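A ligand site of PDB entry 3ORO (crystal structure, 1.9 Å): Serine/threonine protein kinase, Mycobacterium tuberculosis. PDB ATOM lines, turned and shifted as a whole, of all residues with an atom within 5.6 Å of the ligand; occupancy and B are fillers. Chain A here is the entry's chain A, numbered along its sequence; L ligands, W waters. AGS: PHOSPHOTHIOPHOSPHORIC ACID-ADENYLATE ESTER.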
ATOM      1  N   LEU A  20     -17.929  20.192 -17.472  1.00  0.00           N
ATOM      2  CA  LEU A  20     -17.847  19.306 -16.315  1.00  0.00           C
ATOM      3  C   LEU A  20     -18.672  19.773 -15.114  1.00  0.00           C
ATOM      4  O   LEU A  20     -19.222  18.959 -14.370  1.00  0.00           O
ATOM      5  CB  LEU A  20     -16.392  19.148 -15.878  1.00  0.00           C
ATOM      6  CG  LEU A  20     -15.466  18.427 -16.842  1.00  0.00           C
ATOM      7  CD1 LEU A  20     -14.025  18.569 -16.360  1.00  0.00           C
ATOM      8  CD2 LEU A  20     -15.860  16.972 -16.983  1.00  0.00           C
ATOM      9  N   GLY A  21     -18.738  21.082 -14.908  1.00  0.00           N
ATOM     10  CA  GLY A  21     -19.477  21.594 -13.772  1.00  0.00           C
ATOM     11  C   GLY A  21     -19.436  23.094 -13.727  1.00  0.00           C
ATOM     12  O   GLY A  21     -18.820  23.727 -14.579  1.00  0.00           O
ATOM     13  N   PHE A  22     -20.100  23.666 -12.720  1.00  0.00           N
ATOM     14  CA  PHE A  22     -20.056  25.098 -12.476  1.00  0.00           C
ATOM     15  C   PHE A  22     -20.262  25.351 -10.984  1.00  0.00           C
ATOM     16  O   PHE A  22     -20.784  24.498 -10.265  1.00  0.00           O
ATOM     17  CB  PHE A  22     -21.120  25.835 -13.302  1.00  0.00           C
ATOM     18  CG  PHE A  22     -22.533  25.604 -12.832  1.00  0.00           C
ATOM     19  CD1 PHE A  22     -23.190  26.551 -12.075  1.00  0.00           C
ATOM     20  CD2 PHE A  22     -23.196  24.416 -13.143  1.00  0.00           C
ATOM     21  CE1 PHE A  22     -24.503  26.341 -11.634  1.00  0.00           C
ATOM     22  CE2 PHE A  22     -24.498  24.198 -12.704  1.00  0.00           C
ATOM     23  CZ  PHE A  22     -25.143  25.160 -11.952  1.00  0.00           C
ATOM     24  N   GLY A  23     -19.831  26.520 -10.528  1.00  0.00           N
ATOM     25  CA  GLY A  23     -20.045  26.957  -9.156  1.00  0.00           C
ATOM     26  C   GLY A  23     -20.644  28.334  -9.146  1.00  0.00           C
ATOM     27  O   GLY A  23     -21.338  28.723 -10.085  1.00  0.00           O
ATOM     28  N   GLY A  24     -20.383  29.075  -8.075  1.00  0.00           N
ATOM     29  CA  GLY A  24     -20.929  30.418  -7.928  1.00  0.00           C
ATOM     30  C   GLY A  24     -20.349  31.432  -8.901  1.00  0.00           C
ATOM     31  O   GLY A  24     -20.969  32.443  -9.191  1.00  0.00           O
ATOM     32  N   MET A  25     -19.154  31.144  -9.425  1.00  0.00           N
ATOM     33  CA  MET A  25     -18.428  32.081 -10.267  1.00  0.00           C
ATOM     34  C   MET A  25     -18.005  31.513 -11.621  1.00  0.00           C
ATOM     35  O   MET A  25     -18.017  32.232 -12.623  1.00  0.00           O
ATOM     36  CB  MET A  25     -17.176  32.562  -9.528  1.00  0.00           C
ATOM     37  CG  MET A  25     -16.162  33.290 -10.380  1.00  0.00           C
ATOM     38  SD  MET A  25     -14.806  34.017  -9.416  1.00  0.00           S
ATOM     39  CE  MET A  25     -13.921  32.545  -8.897  1.00  0.00           C
ATOM     40  N   SER A  26     -17.602  30.247 -11.642  1.00  0.00           N
ATOM     41  CA  SER A  26     -16.870  29.696 -12.757  1.00  0.00           C
ATOM     42  C   SER A  26     -17.577  28.522 -13.418  1.00  0.00           C
ATOM     43  O   SER A  26     -18.429  27.879 -12.825  1.00  0.00           O
ATOM     44  CB  SER A  26     -15.489  29.222 -12.280  1.00  0.00           C
ATOM     45  OG  SER A  26     -14.853  30.217 -11.499  1.00  0.00           O
ATOM     46  N   GLU A  27     -17.201  28.269 -14.677  1.00  0.00           N
ATOM     47  CA  GLU A  27     -17.574  27.030 -15.354  1.00  0.00           C
ATOM     48  C   GLU A  27     -16.296  26.273 -15.732  1.00  0.00           C
ATOM     49  O   GLU A  27     -15.244  26.880 -16.014  1.00  0.00           O
ATOM     50  CB  GLU A  27     -18.484  27.281 -16.551  1.00  0.00           C
ATOM     51  CG  GLU A  27     -17.908  28.194 -17.615  1.00  0.00           C
ATOM     52  CD  GLU A  27     -18.877  28.415 -18.756  1.00  0.00           C
ATOM     53  OE1 GLU A  27     -18.549  28.015 -19.904  1.00  0.00           O
ATOM     54  OE2 GLU A  27     -19.957  28.998 -18.493  1.00  0.00           O
ATOM     55  N   VAL A  28     -16.371  24.947 -15.699  1.00  0.00           N
ATOM     56  CA  VAL A  28     -15.190  24.101 -15.887  1.00  0.00           C
ATOM     57  C   VAL A  28     -15.471  23.084 -16.996  1.00  0.00           C
ATOM     58  O   VAL A  28     -16.484  22.382 -16.979  1.00  0.00           O
ATOM     59  CB  VAL A  28     -14.803  23.373 -14.571  1.00  0.00           C
ATOM     60  CG1 VAL A  28     -13.537  22.513 -14.772  1.00  0.00           C
ATOM     61  CG2 VAL A  28     -14.592  24.397 -13.437  1.00  0.00           C
ATOM     62  N   ALA A  41      -8.702  19.995 -17.007  1.00  0.00           N
ATOM     63  CA  ALA A  41      -9.919  20.727 -16.739  1.00  0.00           C
ATOM     64  C   ALA A  41      -9.605  22.192 -16.924  1.00  0.00           C
ATOM     65  O   ALA A  41      -8.595  22.684 -16.424  1.00  0.00           O
ATOM     66  CB  ALA A  41     -10.436  20.443 -15.333  1.00  0.00           C
ATOM     67  N   LYS A  43     -10.899  26.001 -16.434  1.00  0.00           N
ATOM     68  CA  LYS A  43     -11.822  26.822 -15.673  1.00  0.00           C
ATOM     69  C   LYS A  43     -11.822  28.261 -16.183  1.00  0.00           C
ATOM     70  O   LYS A  43     -10.759  28.880 -16.315  1.00  0.00           O
ATOM     71  CB  LYS A  43     -11.461  26.819 -14.194  1.00  0.00           C
ATOM     72  CG  LYS A  43     -12.425  27.641 -13.363  1.00  0.00           C
ATOM     73  CD  LYS A  43     -11.834  28.185 -12.123  1.00  0.00           C
ATOM     74  CE  LYS A  43     -11.822  27.207 -11.018  1.00  0.00           C
ATOM     75  NZ  LYS A  43     -11.926  27.947  -9.724  1.00  0.00           N
ATOM     76  N   ARG A  58     -12.734  39.257  -9.270  1.00  0.00           N
ATOM     77  CA  ARG A  58     -12.410  38.134  -8.410  1.00  0.00           C
ATOM     78  C   ARG A  58     -11.743  36.996  -9.193  1.00  0.00           C
ATOM     79  O   ARG A  58     -10.743  36.443  -8.746  1.00  0.00           O
ATOM     80  CB  ARG A  58     -13.658  37.593  -7.700  1.00  0.00           C
ATOM     81  CG  ARG A  58     -13.340  36.396  -6.808  1.00  0.00           C
ATOM     82  CD  ARG A  58     -14.563  35.775  -6.177  1.00  0.00           C
ATOM     83  NE  ARG A  58     -14.190  34.487  -5.584  1.00  0.00           N
ATOM     84  CZ  ARG A  58     -15.007  33.458  -5.393  1.00  0.00           C
ATOM     85  NH1 ARG A  58     -16.288  33.506  -5.703  1.00  0.00           N
ATOM     86  NH2 ARG A  58     -14.515  32.330  -4.872  1.00  0.00           N
ATOM     87  N   PHE A  59     -12.318  36.636 -10.325  1.00  0.00           N
ATOM     88  CA  PHE A  59     -11.774  35.511 -11.099  1.00  0.00           C
ATOM     89  C   PHE A  59     -10.332  35.794 -11.538  1.00  0.00           C
ATOM     90  O   PHE A  59      -9.452  34.940 -11.416  1.00  0.00           O
ATOM     91  CB  PHE A  59     -12.617  35.200 -12.326  1.00  0.00           C
ATOM     92  CG  PHE A  59     -12.230  33.916 -12.996  1.00  0.00           C
ATOM     93  CD1 PHE A  59     -12.933  32.749 -12.739  1.00  0.00           C
ATOM     94  CD2 PHE A  59     -11.118  33.855 -13.847  1.00  0.00           C
ATOM     95  CE1 PHE A  59     -12.568  31.550 -13.346  1.00  0.00           C
ATOM     96  CE2 PHE A  59     -10.743  32.654 -14.434  1.00  0.00           C
ATOM     97  CZ  PHE A  59     -11.458  31.507 -14.184  1.00  0.00           C
ATOM     98  N   VAL A  75      -5.456  19.037  -6.348  1.00  0.00           N
ATOM     99  CA  VAL A  75      -5.648  19.237  -7.783  1.00  0.00           C
ATOM    100  C   VAL A  75      -4.561  20.167  -8.294  1.00  0.00           C
ATOM    101  O   VAL A  75      -4.504  21.332  -7.899  1.00  0.00           O
ATOM    102  CB  VAL A  75      -7.052  19.828  -8.090  1.00  0.00           C
ATOM    103  CG1 VAL A  75      -7.163  20.273  -9.566  1.00  0.00           C
ATOM    104  CG2 VAL A  75      -8.124  18.808  -7.758  1.00  0.00           C
ATOM    105  N   MET A  95      -6.003  22.946 -15.174  1.00  0.00           N
ATOM    106  CA  MET A  95      -5.658  22.103 -14.049  1.00  0.00           C
ATOM    107  C   MET A  95      -5.894  20.607 -14.330  1.00  0.00           C
ATOM    108  O   MET A  95      -6.527  20.218 -15.318  1.00  0.00           O
ATOM    109  CB  MET A  95      -6.449  22.522 -12.800  1.00  0.00           C
ATOM    110  CG  MET A  95      -7.946  22.319 -12.900  1.00  0.00           C
ATOM    111  SD  MET A  95      -8.869  23.158 -11.574  1.00  0.00           S
ATOM    112  CE  MET A  95     -10.335  23.595 -12.502  1.00  0.00           C
ATOM    113  N   GLU A  96      -5.347  19.803 -13.439  1.00  0.00           N
ATOM    114  CA  GLU A  96      -5.560  18.375 -13.396  1.00  0.00           C
ATOM    115  C   GLU A  96      -7.048  18.030 -13.489  1.00  0.00           C
ATOM    116  O   GLU A  96      -7.872  18.615 -12.773  1.00  0.00           O
ATOM    117  CB  GLU A  96      -4.980  17.852 -12.081  1.00  0.00           C
ATOM    118  CG  GLU A  96      -5.128  16.365 -11.827  1.00  0.00           C
ATOM    119  CD  GLU A  96      -4.613  15.968 -10.457  1.00  0.00           C
ATOM    120  OE1 GLU A  96      -5.038  14.898  -9.976  1.00  0.00           O
ATOM    121  OE2 GLU A  96      -3.778  16.702  -9.863  1.00  0.00           O
ATOM    122  N   TYR A  97      -7.392  17.088 -14.369  1.00  0.00           N
ATOM    123  CA  TYR A  97      -8.777  16.636 -14.486  1.00  0.00           C
ATOM    124  C   TYR A  97      -9.072  15.573 -13.422  1.00  0.00           C
ATOM    125  O   TYR A  97      -8.325  14.608 -13.267  1.00  0.00           O
ATOM    126  CB  TYR A  97      -9.056  16.095 -15.898  1.00  0.00           C
ATOM    127  CG  TYR A  97     -10.323  15.281 -16.059  1.00  0.00           C
ATOM    128  CD1 TYR A  97     -11.575  15.801 -15.736  1.00  0.00           C
ATOM    129  CD2 TYR A  97     -10.268  13.980 -16.557  1.00  0.00           C
ATOM    130  CE1 TYR A  97     -12.730  15.036 -15.887  1.00  0.00           C
ATOM    131  CE2 TYR A  97     -11.407  13.226 -16.721  1.00  0.00           C
ATOM    132  CZ  TYR A  97     -12.638  13.760 -16.384  1.00  0.00           C
ATOM    133  OH  TYR A  97     -13.754  12.977 -16.544  1.00  0.00           O
ATOM    134  N   VAL A  98     -10.171  15.763 -12.699  1.00  0.00           N
ATOM    135  CA  VAL A  98     -10.656  14.762 -11.753  1.00  0.00           C
ATOM    136  C   VAL A  98     -11.958  14.178 -12.283  1.00  0.00           C
ATOM    137  O   VAL A  98     -12.958  14.889 -12.409  1.00  0.00           O
ATOM    138  CB  VAL A  98     -10.925  15.370 -10.364  1.00  0.00           C
ATOM    139  CG1 VAL A  98     -11.351  14.255  -9.407  1.00  0.00           C
ATOM    140  CG2 VAL A  98      -9.709  16.102  -9.842  1.00  0.00           C
ATOM    141  N   ASP A  99     -11.938  12.893 -12.642  1.00  0.00           N
ATOM    142  CA  ASP A  99     -13.141  12.169 -12.984  1.00  0.00           C
ATOM    143  C   ASP A  99     -13.811  11.759 -11.685  1.00  0.00           C
ATOM    144  O   ASP A  99     -13.397  10.795 -11.050  1.00  0.00           O
ATOM    145  CB  ASP A  99     -12.816  10.927 -13.826  1.00  0.00           C
ATOM    146  CG  ASP A  99     -14.050  10.131 -14.225  1.00  0.00           C
ATOM    147  OD1 ASP A  99     -15.197  10.611 -14.044  1.00  0.00           O
ATOM    148  OD2 ASP A  99     -13.882   9.002 -14.729  1.00  0.00           O
ATOM    149  N   THR A 102     -17.953  16.051  -6.185  1.00  0.00           N
ATOM    150  CA  THR A 102     -17.581  16.759  -4.963  1.00  0.00           C
ATOM    151  C   THR A 102     -18.280  16.131  -3.743  1.00  0.00           C
ATOM    152  O   THR A 102     -19.295  15.437  -3.874  1.00  0.00           O
ATOM    153  CB  THR A 102     -17.960  18.257  -5.040  1.00  0.00           C
ATOM    154  OG1 THR A 102     -19.373  18.384  -4.977  1.00  0.00           O
ATOM    155  CG2 THR A 102     -17.444  18.896  -6.316  1.00  0.00           C
ATOM    156  N   ASP A 105     -21.884  17.072  -3.764  1.00  0.00           N
ATOM    157  CA  ASP A 105     -22.648  16.137  -4.606  1.00  0.00           C
ATOM    158  C   ASP A 105     -23.003  14.859  -3.855  1.00  0.00           C
ATOM    159  O   ASP A 105     -24.131  14.379  -3.920  1.00  0.00           O
ATOM    160  CB  ASP A 105     -21.855  15.707  -5.846  1.00  0.00           C
ATOM    161  CG  ASP A 105     -21.610  16.840  -6.837  1.00  0.00           C
ATOM    162  OD1 ASP A 105     -22.453  17.757  -6.918  1.00  0.00           O
ATOM    163  OD2 ASP A 105     -20.576  16.781  -7.572  1.00  0.00           O
ATOM    164  N   ASP A 141     -10.932  28.537   2.106  1.00  0.00           N
ATOM    165  CA  ASP A 141     -12.283  28.218   1.626  1.00  0.00           C
ATOM    166  C   ASP A 141     -12.548  26.711   1.619  1.00  0.00           C
ATOM    167  O   ASP A 141     -13.101  26.167   0.641  1.00  0.00           O
ATOM    168  CB  ASP A 141     -12.491  28.778   0.222  1.00  0.00           C
ATOM    169  CG  ASP A 141     -13.963  28.760  -0.213  1.00  0.00           C
ATOM    170  OD1 ASP A 141     -14.864  29.090   0.603  1.00  0.00           O
ATOM    171  OD2 ASP A 141     -14.201  28.389  -1.382  1.00  0.00           O
ATOM    172  N   LYS A 143     -14.597  23.647   2.127  1.00  0.00           N
ATOM    173  CA  LYS A 143     -16.027  23.365   2.136  1.00  0.00           C
ATOM    174  C   LYS A 143     -16.279  22.114   1.280  1.00  0.00           C
ATOM    175  O   LYS A 143     -15.391  21.701   0.535  1.00  0.00           O
ATOM    176  CB  LYS A 143     -16.843  24.556   1.599  1.00  0.00           C
ATOM    177  CG  LYS A 143     -16.483  24.982   0.168  1.00  0.00           C
ATOM    178  CD  LYS A 143     -17.320  26.142  -0.309  1.00  0.00           C
ATOM    179  CE  LYS A 143     -17.071  26.426  -1.805  1.00  0.00           C
ATOM    180  NZ  LYS A 143     -17.538  27.791  -2.197  1.00  0.00           N
ATOM    181  N   ALA A 145     -17.919  21.459  -1.426  1.00  0.00           N
ATOM    182  CA  ALA A 145     -17.761  21.647  -2.865  1.00  0.00           C
ATOM    183  C   ALA A 145     -16.314  21.748  -3.352  1.00  0.00           C
ATOM    184  O   ALA A 145     -16.059  21.584  -4.558  1.00  0.00           O
ATOM    185  CB  ALA A 145     -18.550  22.848  -3.344  1.00  0.00           C
ATOM    186  N   ASN A 146     -15.357  21.994  -2.450  1.00  0.00           N
ATOM    187  CA  ASN A 146     -13.948  22.133  -2.814  1.00  0.00           C
ATOM    188  C   ASN A 146     -13.087  20.891  -2.555  1.00  0.00           C
ATOM    189  O   ASN A 146     -11.850  20.949  -2.628  1.00  0.00           O
ATOM    190  CB  ASN A 146     -13.337  23.379  -2.141  1.00  0.00           C
ATOM    191  CG  ASN A 146     -13.742  24.648  -2.827  1.00  0.00           C
ATOM    192  OD1 ASN A 146     -14.209  24.622  -3.980  1.00  0.00           O
ATOM    193  ND2 ASN A 146     -13.598  25.787  -2.143  1.00  0.00           N
ATOM    194  N   MET A 148     -13.034  16.865  -3.934  1.00  0.00           N
ATOM    195  CA  MET A 148     -13.578  15.838  -4.816  1.00  0.00           C
ATOM    196  C   MET A 148     -13.121  14.440  -4.433  1.00  0.00           C
ATOM    197  O   MET A 148     -12.075  14.265  -3.796  1.00  0.00           O
ATOM    198  CB  MET A 148     -13.215  16.124  -6.285  1.00  0.00           C
ATOM    199  CG  MET A 148     -13.858  17.403  -6.834  1.00  0.00           C
ATOM    200  SD  MET A 148     -13.619  17.715  -8.595  1.00  0.00           S
ATOM    201  CE  MET A 148     -14.781  16.564  -9.336  1.00  0.00           C
ATOM    202  N   MET A 158      -9.263  21.076  -3.777  1.00  0.00           N
ATOM    203  CA  MET A 158      -9.052  22.063  -4.832  1.00  0.00           C
ATOM    204  C   MET A 158      -9.490  23.476  -4.486  1.00  0.00           C
ATOM    205  O   MET A 158     -10.054  23.729  -3.420  1.00  0.00           O
ATOM    206  CB  MET A 158      -9.762  21.594  -6.099  1.00  0.00           C
ATOM    207  CG  MET A 158     -11.256  21.700  -6.049  1.00  0.00           C
ATOM    208  SD  MET A 158     -11.995  20.709  -7.355  1.00  0.00           S
ATOM    209  CE  MET A 158     -13.717  21.180  -7.173  1.00  0.00           C
ATOM    210  N   ASP A 159      -9.210  24.372  -5.424  1.00  0.00           N
ATOM    211  CA  ASP A 159      -9.696  25.745  -5.370  1.00  0.00           C
ATOM    212  C   ASP A 159      -9.228  26.450  -4.100  1.00  0.00           C
ATOM    213  O   ASP A 159     -10.026  27.027  -3.353  1.00  0.00           O
ATOM    214  CB  ASP A 159     -11.225  25.781  -5.509  1.00  0.00           C
ATOM    215  CG  ASP A 159     -11.746  27.157  -5.947  1.00  0.00           C
ATOM    216  OD1 ASP A 159     -10.950  27.953  -6.460  1.00  0.00           O
ATOM    217  OD2 ASP A 159     -12.947  27.424  -5.757  1.00  0.00           O
ATOM    218  N   ALA A 177     -19.534  38.750  -5.016  1.00  0.00           N
ATOM    219  CA  ALA A 177     -18.881  37.877  -6.000  1.00  0.00           C
ATOM    220  C   ALA A 177     -18.844  36.432  -5.507  1.00  0.00           C
ATOM    221  O   ALA A 177     -17.900  35.700  -5.790  1.00  0.00           O
ATOM    222  CB  ALA A 177     -17.484  38.378  -6.319  1.00  0.00           C
ATOM    223  N   ALA A 178     -19.876  36.024  -4.766  1.00  0.00           N
ATOM    224  CA  ALA A 178     -19.999  34.641  -4.273  1.00  0.00           C
ATOM    225  C   ALA A 178     -18.878  34.206  -3.319  1.00  0.00           C
ATOM    226  O   ALA A 178     -18.697  33.011  -3.082  1.00  0.00           O
ATOM    227  CB  ALA A 178     -20.116  33.659  -5.467  1.00  0.00           C
HETATM  228  PG  AGS L   1     -17.234  28.505  -5.963  1.00  0.00           P
HETATM  229  S1G AGS L   1     -17.488  30.222  -5.980  1.00  0.00           S
HETATM  230  O2G AGS L   1     -18.562  27.760  -6.159  1.00  0.00           O
HETATM  231  O3G AGS L   1     -16.584  27.974  -4.674  1.00  0.00           O
HETATM  232  PB  AGS L   1     -16.161  28.260  -8.698  1.00  0.00           P
HETATM  233  O1B AGS L   1     -17.453  28.757  -9.223  1.00  0.00           O
HETATM  234  O2B AGS L   1     -14.946  29.089  -9.121  1.00  0.00           O
HETATM  235  O3B AGS L   1     -16.179  28.049  -7.087  1.00  0.00           O
HETATM  236  PA  AGS L   1     -15.092  25.542  -8.739  1.00  0.00           P
HETATM  237  O1A AGS L   1     -13.630  25.727  -8.952  1.00  0.00           O
HETATM  238  O2A AGS L   1     -15.487  25.060  -7.366  1.00  0.00           O
HETATM  239  O3A AGS L   1     -15.997  26.770  -9.278  1.00  0.00           O
HETATM  240  O5' AGS L   1     -15.624  24.448  -9.816  1.00  0.00           O
HETATM  241  C5' AGS L   1     -17.013  24.261 -10.027  1.00  0.00           C
HETATM  242  C4' AGS L   1     -17.288  22.828 -10.445  1.00  0.00           C
HETATM  243  O4' AGS L   1     -16.553  22.502 -11.600  1.00  0.00           O
HETATM  244  C3' AGS L   1     -16.909  21.801  -9.389  1.00  0.00           C
HETATM  245  O3' AGS L   1     -17.891  21.652  -8.381  1.00  0.00           O
HETATM  246  C2' AGS L   1     -16.745  20.578 -10.257  1.00  0.00           C
HETATM  247  O2' AGS L   1     -17.991  20.005 -10.574  1.00  0.00           O
HETATM  248  C1' AGS L   1     -16.118  21.146 -11.510  1.00  0.00           C
HETATM  249  N9  AGS L   1     -14.653  21.106 -11.412  1.00  0.00           N
HETATM  250  C8  AGS L   1     -13.827  22.068 -10.877  1.00  0.00           C
HETATM  251  N7  AGS L   1     -12.557  21.631 -10.964  1.00  0.00           N
HETATM  252  C5  AGS L   1     -12.560  20.419 -11.559  1.00  0.00           C
HETATM  253  C6  AGS L   1     -11.532  19.525 -11.892  1.00  0.00           C
HETATM  254  N6  AGS L   1     -10.258  19.809 -11.631  1.00  0.00           N
HETATM  255  N1  AGS L   1     -11.873  18.347 -12.503  1.00  0.00           N
HETATM  256  C2  AGS L   1     -13.188  18.013 -12.777  1.00  0.00           C
HETATM  257  N3  AGS L   1     -14.209  18.879 -12.436  1.00  0.00           N
HETATM  258  C4  AGS L   1     -13.886  20.069 -11.828  1.00  0.00           C
HETATM  259  O   HOH W   1     -16.811  23.256  -6.409  1.00  0.00           O
HETATM  260  O   HOH W   2     -11.481  23.851  -9.183  1.00  0.00           O
HETATM  261  O   HOH W   3     -20.350  28.885  -4.419  1.00  0.00           O
HETATM  262  O   HOH W   4     -20.584  21.379  -8.520  1.00  0.00           O
HETATM  263  O   HOH W   5     -16.695  17.723 -12.373  1.00  0.00           O
HETATM  264  O   HOH W   6     -18.999  25.070  -6.183  1.00  0.00           O
HETATM  265  O   HOH W   7     -16.895  31.041  -2.893  1.00  0.00           O
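The side-chain amino group of Lys 143 is in hydrogen-bond range of an oxygen (O3G) of the ligand. The side-chain amino group (NZ) of Lys 43 lies within salt-bridge range of an oxygen (O1A) of the ligand, 2.9 Å away. N6 of the ligand sits at hydrogen-bond distance from SD of Met 95 (3.6 Å). A nitrogen (N6) of the ligand lies within hydrogen-bond range of the backbone carbonyl oxygen of Glu 96 (2.9 Å). An oxygen (O1B) of the ligand is in hydrogen-bond range of the backbone NH of Ser 26, at 2.8 Å. OG of Ser 26 sits at hydrogen-bond distance from O2B of the ligand. N of Met 25 sits at hydrogen-bond distance from O1B of the ligand, 2.9 Å away. The guanidinium group of Arg 58 sits close to a sulfur (S1G) of the ligand. N1 of the ligand lies within hydrogen-bond range of N of Val 98 (3.1 Å). The backbone NH (N) of Gly 24 lies within hydrogen-bond range of an oxygen (O2G) of the ligand.
NH1 of Arg 58 is in hydrogen-bond range of O of Ala 177. SD of Met 25 lies within hydrogen-bond range of N of Phe 59 (3.7 Å). NZ of Lys 143 lies within salt-bridge range of OD2 of Asp 141 (3.5 Å). N of Val 28 lies within hydrogen-bond range of O of Gly 21 (3.0 Å). The backbone NH (N) of Thr 102 lies within hydrogen-bond range of the side-chain carboxylate (OD2) of Asp 105 (3.1 Å). The backbone carbonyl oxygen (O) of Met 95 sits at hydrogen-bond distance from the backbone NH (N) of Ala 41, at 2.8 Å. NZ of Lys 43 is in salt-bridge range of OD1 of Asp 159. The backbone carbonyl oxygen (O) of Asn 146 is in hydrogen-bond range of the backbone NH (N) of Met 158 (2.8 Å).
The side-chain sulfur (SD) of Met 158 sits close to a nitrogen (N7) of the ligand (3.8 Å). Leu 20 touches the ligand. C of Gly 21 touches O4' of the ligand, 3.6 Å away. Phe 22 touches the ligand. CA of Gly 23 touches O1B of the ligand, at 3.2 Å. Val 28 touches the ligand (CG2 to O4', 3.3 Å). CB of Ala 41 touches C6 of the ligand, 3.7 Å away. Val 75 touches the ligand (CG1 to N6, 3.7 Å). Thr 102 touches the ligand. OD1 of Asn 146 touches O2A of the ligand (3.6 Å). CE of Met 148 touches N3 of the ligand, 3.9 Å away. Asp 159 touches the ligand. Hydrophobic or aromatic side chains within 4 Å of the ligand: Leu 20, Met 25, Val 28, Ala 41, Val 75, Met 95, Val 98, Met 148 and Met 158.
Water W1 bridges O2A of the ligand and O of Ala 145. Water W5 bridges N3 of the ligand (2.7 Å) and O of Leu 20 (3.4 Å). Water W2 lies within hydrogen-bond range of O1A of the ligand (2.9 Å), SD of Met 95 (3.6 Å) and SD of Met 158 (3.7 Å). Water W7 lies within hydrogen-bond range of the backbone carbonyl oxygen of Ala 178 (2.7 Å), a sulfur (S1G) of the ligand (3.2 Å), the guanidinium group of Arg 58 (3.4 Å) and the side-chain amino group of Lys 143 (3.4 Å).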
